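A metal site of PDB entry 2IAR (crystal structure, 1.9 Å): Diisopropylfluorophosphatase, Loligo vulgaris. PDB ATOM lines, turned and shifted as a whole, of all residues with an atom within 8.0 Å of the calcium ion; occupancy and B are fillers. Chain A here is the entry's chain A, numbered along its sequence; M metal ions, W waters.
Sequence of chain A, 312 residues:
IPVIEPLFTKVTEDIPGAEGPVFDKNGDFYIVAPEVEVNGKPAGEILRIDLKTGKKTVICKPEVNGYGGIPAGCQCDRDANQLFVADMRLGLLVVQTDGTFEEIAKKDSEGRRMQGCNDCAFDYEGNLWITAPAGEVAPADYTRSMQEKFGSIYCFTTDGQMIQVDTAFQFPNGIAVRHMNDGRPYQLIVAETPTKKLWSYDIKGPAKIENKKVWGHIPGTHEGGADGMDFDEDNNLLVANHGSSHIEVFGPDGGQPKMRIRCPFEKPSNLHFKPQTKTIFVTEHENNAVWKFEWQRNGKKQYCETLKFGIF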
ATOM      1  N   GLU A  19     -16.458 -18.369 -24.468  1.00  0.00           N
ATOM      2  CA  GLU A  19     -15.883 -17.862 -23.235  1.00  0.00           C
ATOM      3  C   GLU A  19     -14.676 -18.623 -22.696  1.00  0.00           C
ATOM      4  O   GLU A  19     -14.237 -19.624 -23.269  1.00  0.00           O
ATOM      5  CB  GLU A  19     -16.970 -17.893 -22.141  1.00  0.00           C
ATOM      6  CG  GLU A  19     -17.677 -16.580 -21.906  1.00  0.00           C
ATOM      7  CD  GLU A  19     -16.950 -15.702 -20.917  1.00  0.00           C
ATOM      8  OE1 GLU A  19     -15.711 -15.811 -20.778  1.00  0.00           O
ATOM      9  OE2 GLU A  19     -17.633 -14.911 -20.248  1.00  0.00           O
ATOM     10  N   GLY A  20     -14.202 -18.134 -21.554  1.00  0.00           N
ATOM     11  CA  GLY A  20     -13.088 -18.705 -20.819  1.00  0.00           C
ATOM     12  C   GLY A  20     -11.905 -19.305 -21.531  1.00  0.00           C
ATOM     13  O   GLY A  20     -11.542 -20.441 -21.211  1.00  0.00           O
ATOM     14  N   PRO A  21     -11.245 -18.577 -22.456  1.00  0.00           N
ATOM     15  CA  PRO A  21     -10.083 -19.127 -23.176  1.00  0.00           C
ATOM     16  C   PRO A  21      -8.981 -19.459 -22.169  1.00  0.00           C
ATOM     17  O   PRO A  21      -8.738 -18.706 -21.215  1.00  0.00           O
ATOM     18  CB  PRO A  21      -9.693 -17.988 -24.117  1.00  0.00           C
ATOM     19  CG  PRO A  21     -10.094 -16.764 -23.370  1.00  0.00           C
ATOM     20  CD  PRO A  21     -11.453 -17.164 -22.827  1.00  0.00           C
ATOM     21  N   VAL A  22      -8.328 -20.588 -22.364  1.00  0.00           N
ATOM     22  CA  VAL A  22      -7.276 -21.006 -21.451  1.00  0.00           C
ATOM     23  C   VAL A  22      -6.316 -22.014 -22.080  1.00  0.00           C
ATOM     24  O   VAL A  22      -6.674 -22.750 -23.002  1.00  0.00           O
ATOM     25  CB  VAL A  22      -7.898 -21.610 -20.149  1.00  0.00           C
ATOM     26  CG1 VAL A  22      -8.502 -22.985 -20.440  1.00  0.00           C
ATOM     27  CG2 VAL A  22      -6.860 -21.675 -19.025  1.00  0.00           C
ATOM     28  N   PHE A  23      -5.091 -21.984 -21.591  1.00  0.00           N
ATOM     29  CA  PHE A  23      -4.050 -22.913 -22.033  1.00  0.00           C
ATOM     30  C   PHE A  23      -3.705 -23.779 -20.830  1.00  0.00           C
ATOM     31  O   PHE A  23      -3.620 -23.279 -19.704  1.00  0.00           O
ATOM     32  CB  PHE A  23      -2.799 -22.152 -22.463  1.00  0.00           C
ATOM     33  CG  PHE A  23      -2.875 -21.614 -23.862  1.00  0.00           C
ATOM     34  CD1 PHE A  23      -3.277 -20.300 -24.091  1.00  0.00           C
ATOM     35  CD2 PHE A  23      -2.517 -22.406 -24.940  1.00  0.00           C
ATOM     36  CE1 PHE A  23      -3.319 -19.789 -25.379  1.00  0.00           C
ATOM     37  CE2 PHE A  23      -2.559 -21.913 -26.238  1.00  0.00           C
ATOM     38  CZ  PHE A  23      -2.952 -20.592 -26.459  1.00  0.00           C
ATOM     39  N   GLY A  73     -16.001 -19.571 -17.318  1.00  0.00           N
ATOM     40  CA  GLY A  73     -14.642 -19.107 -17.083  1.00  0.00           C
ATOM     41  C   GLY A  73     -13.698 -20.226 -16.695  1.00  0.00           C
ATOM     42  O   GLY A  73     -14.123 -21.203 -16.071  1.00  0.00           O
ATOM     43  N   CYS A  74     -12.417 -20.073 -17.016  1.00  0.00           N
ATOM     44  CA  CYS A  74     -11.430 -21.113 -16.713  1.00  0.00           C
ATOM     45  C   CYS A  74     -10.076 -20.610 -16.215  1.00  0.00           C
ATOM     46  O   CYS A  74      -9.658 -19.476 -16.502  1.00  0.00           O
ATOM     47  CB  CYS A  74     -11.143 -21.968 -17.967  1.00  0.00           C
ATOM     48  SG  CYS A  74     -12.538 -22.629 -18.885  1.00  0.00           S
ATOM     49  N   GLN A  75      -9.387 -21.502 -15.511  1.00  0.00           N
ATOM     50  CA  GLN A  75      -8.039 -21.305 -14.975  1.00  0.00           C
ATOM     51  C   GLN A  75      -7.419 -22.687 -14.957  1.00  0.00           C
ATOM     52  O   GLN A  75      -8.126 -23.678 -14.718  1.00  0.00           O
ATOM     53  CB  GLN A  75      -8.059 -20.765 -13.544  1.00  0.00           C
ATOM     54  CG  GLN A  75      -8.365 -19.298 -13.429  1.00  0.00           C
ATOM     55  CD  GLN A  75      -7.276 -18.418 -14.012  1.00  0.00           C
ATOM     56  OE1 GLN A  75      -7.397 -17.935 -15.143  1.00  0.00           O
ATOM     57  NE2 GLN A  75      -6.233 -18.184 -13.247  1.00  0.00           N
ATOM     58  N   ASP A 119     -16.340 -16.430 -13.699  1.00  0.00           N
ATOM     59  CA  ASP A 119     -14.918 -16.434 -13.983  1.00  0.00           C
ATOM     60  C   ASP A 119     -14.126 -16.600 -12.692  1.00  0.00           C
ATOM     61  O   ASP A 119     -14.661 -16.383 -11.601  1.00  0.00           O
ATOM     62  CB  ASP A 119     -14.497 -15.150 -14.711  1.00  0.00           C
ATOM     63  CG  ASP A 119     -13.295 -15.349 -15.636  1.00  0.00           C
ATOM     64  OD1 ASP A 119     -12.636 -16.400 -15.579  1.00  0.00           O
ATOM     65  OD2 ASP A 119     -13.027 -14.453 -16.446  1.00  0.00           O
ATOM     66  N   CYS A 120     -12.855 -16.969 -12.827  1.00  0.00           N
ATOM     67  CA  CYS A 120     -11.997 -17.196 -11.675  1.00  0.00           C
ATOM     68  C   CYS A 120     -10.546 -16.832 -11.966  1.00  0.00           C
ATOM     69  O   CYS A 120     -10.121 -16.803 -13.130  1.00  0.00           O
ATOM     70  CB  CYS A 120     -12.084 -18.656 -11.214  1.00  0.00           C
ATOM     71  SG  CYS A 120     -11.785 -19.884 -12.495  1.00  0.00           S
ATOM     72  N   ILE A 175     -12.172 -11.298 -13.286  1.00  0.00           N
ATOM     73  CA  ILE A 175     -11.453 -11.163 -12.022  1.00  0.00           C
ATOM     74  C   ILE A 175      -9.971 -11.426 -12.251  1.00  0.00           C
ATOM     75  O   ILE A 175      -9.596 -12.196 -13.140  1.00  0.00           O
ATOM     76  CB  ILE A 175     -12.077 -12.138 -10.959  1.00  0.00           C
ATOM     77  CG1 ILE A 175     -11.439 -11.943  -9.576  1.00  0.00           C
ATOM     78  CG2 ILE A 175     -12.007 -13.574 -11.441  1.00  0.00           C
ATOM     79  CD1 ILE A 175     -12.212 -12.609  -8.471  1.00  0.00           C
ATOM     80  N   GLY A 228     -14.177 -10.102 -19.359  1.00  0.00           N
ATOM     81  CA  GLY A 228     -12.950 -10.784 -18.964  1.00  0.00           C
ATOM     82  C   GLY A 228     -11.732  -9.892 -18.801  1.00  0.00           C
ATOM     83  O   GLY A 228     -11.663  -8.816 -19.393  1.00  0.00           O
ATOM     84  N   MET A 229     -10.762 -10.350 -18.018  1.00  0.00           N
ATOM     85  CA  MET A 229      -9.549  -9.571 -17.774  1.00  0.00           C
ATOM     86  C   MET A 229      -8.316 -10.420 -17.491  1.00  0.00           C
ATOM     87  O   MET A 229      -8.421 -11.592 -17.137  1.00  0.00           O
ATOM     88  CB  MET A 229      -9.760  -8.587 -16.611  1.00  0.00           C
ATOM     89  CG  MET A 229      -9.971  -9.263 -15.267  1.00  0.00           C
ATOM     90  SD  MET A 229     -10.127  -8.115 -13.883  1.00  0.00           S
ATOM     91  CE  MET A 229     -11.561  -7.211 -14.369  1.00  0.00           C
ATOM     92  N   ASP A 230      -7.152  -9.787 -17.602  1.00  0.00           N
ATOM     93  CA  ASP A 230      -5.848 -10.403 -17.369  1.00  0.00           C
ATOM     94  C   ASP A 230      -4.749  -9.344 -17.363  1.00  0.00           C
ATOM     95  O   ASP A 230      -4.862  -8.318 -18.049  1.00  0.00           O
ATOM     96  CB  ASP A 230      -5.511 -11.408 -18.475  1.00  0.00           C
ATOM     97  CG  ASP A 230      -5.860 -12.853 -18.121  1.00  0.00           C
ATOM     98  OD1 ASP A 230      -5.814 -13.240 -16.934  1.00  0.00           O
ATOM     99  OD2 ASP A 230      -6.148 -13.599 -19.066  1.00  0.00           O
ATOM    100  N   PHE A 231      -3.668  -9.617 -16.650  1.00  0.00           N
ATOM    101  CA  PHE A 231      -2.529  -8.715 -16.566  1.00  0.00           C
ATOM    102  C   PHE A 231      -1.428  -9.115 -17.559  1.00  0.00           C
ATOM    103  O   PHE A 231      -1.294 -10.298 -17.900  1.00  0.00           O
ATOM    104  CB  PHE A 231      -1.915  -8.781 -15.164  1.00  0.00           C
ATOM    105  CG  PHE A 231      -2.684  -8.021 -14.123  1.00  0.00           C
ATOM    106  CD1 PHE A 231      -3.365  -8.706 -13.111  1.00  0.00           C
ATOM    107  CD2 PHE A 231      -2.700  -6.624 -14.114  1.00  0.00           C
ATOM    108  CE1 PHE A 231      -4.045  -8.005 -12.112  1.00  0.00           C
ATOM    109  CE2 PHE A 231      -3.380  -5.922 -13.116  1.00  0.00           C
ATOM    110  CZ  PHE A 231      -4.049  -6.623 -12.118  1.00  0.00           C
ATOM    111  N   ASN A 270     -13.872 -12.468 -23.498  1.00  0.00           N
ATOM    112  CA  ASN A 270     -12.767 -12.833 -22.618  1.00  0.00           C
ATOM    113  C   ASN A 270     -11.473 -12.925 -23.408  1.00  0.00           C
ATOM    114  O   ASN A 270     -11.480 -12.914 -24.636  1.00  0.00           O
ATOM    115  CB  ASN A 270     -13.068 -14.185 -21.936  1.00  0.00           C
ATOM    116  CG  ASN A 270     -12.656 -14.212 -20.455  1.00  0.00           C
ATOM    117  OD1 ASN A 270     -13.338 -14.822 -19.621  1.00  0.00           O
ATOM    118  ND2 ASN A 270     -11.538 -13.575 -20.134  1.00  0.00           N
ATOM    119  N   LEU A 271     -10.350 -12.991 -22.699  1.00  0.00           N
ATOM    120  CA  LEU A 271      -9.038 -13.063 -23.337  1.00  0.00           C
ATOM    121  C   LEU A 271      -8.060 -13.888 -22.530  1.00  0.00           C
ATOM    122  O   LEU A 271      -8.299 -14.154 -21.353  1.00  0.00           O
ATOM    123  CB  LEU A 271      -8.485 -11.646 -23.581  1.00  0.00           C
ATOM    124  CG  LEU A 271      -8.432 -10.594 -22.462  1.00  0.00           C
ATOM    125  CD1 LEU A 271      -7.322 -10.893 -21.495  1.00  0.00           C
ATOM    126  CD2 LEU A 271      -8.180  -9.239 -23.090  1.00  0.00           C
ATOM    127  N   HIS A 272      -6.954 -14.286 -23.154  1.00  0.00           N
ATOM    128  CA  HIS A 272      -5.939 -15.077 -22.472  1.00  0.00           C
ATOM    129  C   HIS A 272      -4.651 -15.066 -23.282  1.00  0.00           C
ATOM    130  O   HIS A 272      -4.674 -15.185 -24.502  1.00  0.00           O
ATOM    131  CB  HIS A 272      -6.406 -16.533 -22.284  1.00  0.00           C
ATOM    132  CG  HIS A 272      -5.821 -17.216 -21.085  1.00  0.00           C
ATOM    133  ND1 HIS A 272      -6.242 -16.950 -19.795  1.00  0.00           N
ATOM    134  CD2 HIS A 272      -4.860 -18.163 -20.974  1.00  0.00           C
ATOM    135  CE1 HIS A 272      -5.574 -17.711 -18.955  1.00  0.00           C
ATOM    136  NE2 HIS A 272      -4.728 -18.460 -19.640  1.00  0.00           N
ATOM    137  N   PHE A 273      -3.531 -14.895 -22.591  1.00  0.00           N
ATOM    138  CA  PHE A 273      -2.223 -14.875 -23.230  1.00  0.00           C
ATOM    139  C   PHE A 273      -1.693 -16.292 -23.440  1.00  0.00           C
ATOM    140  O   PHE A 273      -1.952 -17.190 -22.627  1.00  0.00           O
ATOM    141  CB  PHE A 273      -1.202 -14.158 -22.347  1.00  0.00           C
ATOM    142  CG  PHE A 273      -1.250 -12.658 -22.442  1.00  0.00           C
ATOM    143  CD1 PHE A 273      -2.066 -11.911 -21.587  1.00  0.00           C
ATOM    144  CD2 PHE A 273      -0.403 -11.983 -23.314  1.00  0.00           C
ATOM    145  CE1 PHE A 273      -2.044 -10.515 -21.598  1.00  0.00           C
ATOM    146  CE2 PHE A 273      -0.370 -10.573 -23.350  1.00  0.00           C
ATOM    147  CZ  PHE A 273      -1.194  -9.843 -22.484  1.00  0.00           C
ATOM    148  N   ILE A 280      -2.564 -12.713 -27.699  1.00  0.00           N
ATOM    149  CA  ILE A 280      -3.761 -12.722 -26.873  1.00  0.00           C
ATOM    150  C   ILE A 280      -4.909 -13.319 -27.660  1.00  0.00           C
ATOM    151  O   ILE A 280      -5.254 -12.843 -28.734  1.00  0.00           O
ATOM    152  CB  ILE A 280      -4.169 -11.314 -26.419  1.00  0.00           C
ATOM    153  CG1 ILE A 280      -3.136 -10.740 -25.462  1.00  0.00           C
ATOM    154  CG2 ILE A 280      -5.515 -11.358 -25.714  1.00  0.00           C
ATOM    155  CD1 ILE A 280      -3.513  -9.374 -24.933  1.00  0.00           C
ATOM    156  N   PHE A 281      -5.485 -14.387 -27.115  1.00  0.00           N
ATOM    157  CA  PHE A 281      -6.635 -15.064 -27.716  1.00  0.00           C
ATOM    158  C   PHE A 281      -7.884 -14.402 -27.157  1.00  0.00           C
ATOM    159  O   PHE A 281      -8.023 -14.247 -25.939  1.00  0.00           O
ATOM    160  CB  PHE A 281      -6.579 -16.560 -27.420  1.00  0.00           C
ATOM    161  CG  PHE A 281      -5.563 -17.297 -28.255  1.00  0.00           C
ATOM    162  CD1 PHE A 281      -5.963 -18.060 -29.356  1.00  0.00           C
ATOM    163  CD2 PHE A 281      -4.195 -17.181 -27.987  1.00  0.00           C
ATOM    164  CE1 PHE A 281      -5.010 -18.681 -30.193  1.00  0.00           C
ATOM    165  CE2 PHE A 281      -3.237 -17.809 -28.812  1.00  0.00           C
ATOM    166  CZ  PHE A 281      -3.656 -18.559 -29.914  1.00  0.00           C
ATOM    167  N   GLN A 302       0.609 -17.157 -15.559  1.00  0.00           N
ATOM    168  CA  GLN A 302      -0.545 -17.680 -14.835  1.00  0.00           C
ATOM    169  C   GLN A 302       0.007 -18.600 -13.766  1.00  0.00           C
ATOM    170  O   GLN A 302       1.146 -19.038 -13.837  1.00  0.00           O
ATOM    171  CB  GLN A 302      -1.438 -18.473 -15.789  1.00  0.00           C
ATOM    172  CG  GLN A 302      -2.268 -17.628 -16.739  1.00  0.00           C
ATOM    173  CD  GLN A 302      -3.482 -17.029 -16.065  1.00  0.00           C
ATOM    174  OE1 GLN A 302      -3.474 -15.866 -15.649  1.00  0.00           O
ATOM    175  NE2 GLN A 302      -4.539 -17.817 -15.942  1.00  0.00           N
HETATM  176 CA    CA M   1      -8.032 -15.238 -19.230  1.00  0.00          CA
HETATM  177  O   HOH W   1      -7.440 -15.461 -16.790  1.00  0.00           O
HETATM  178  O   HOH W   2      -9.958 -16.697 -19.972  1.00  0.00           O
HETATM  179  O   HOH W   3      -9.657 -13.644 -18.328  1.00  0.00           O
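ND1 of His 272 sits close to O of Pro 21, at 3.4 Å.
N of Phe 281 is in hydrogen-bond range of O of His 272 (2.8 Å).
OD1 of Asn 270 sits close to OD2 of Asp 119 (3.2 Å).
The side-chain carboxylate (OE1) of Glu 19 lies close to the side-chain amide oxygen (OD1) of Asn 270, at 2.8 Å.
Asn 270 touches the calcium ion (ND2 to CA, 3.98 Å).
Four residues have an atom within 4 Å of the calcium ion: Asp 230, Asn 270, Leu 271 and His 272.
Along chain A the residues within 4 Å of the calcium ion span positions 230 to 272.
Water W3 bridges the side-chain amide nitrogen (ND2) of Asn 270 (2.6 Å) and the backbone carbonyl oxygen (O) of Met 229 (2.7 Å).
Water W1 bridges the side-chain carboxylate (OD1) of Asp 230 and the side-chain amide oxygen (OE1) of Gln 75.
The calcium ion is bound by O of Leu 271 (2.4 Å), water W3 (2.4 Å), OD2 of Asp 230 (2.5 Å), water W1 (2.5 Å), water W2 (2.5 Å) and ND1 of His 272 (2.5 Å).
The calcium ion has six donor atoms within binding distance.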
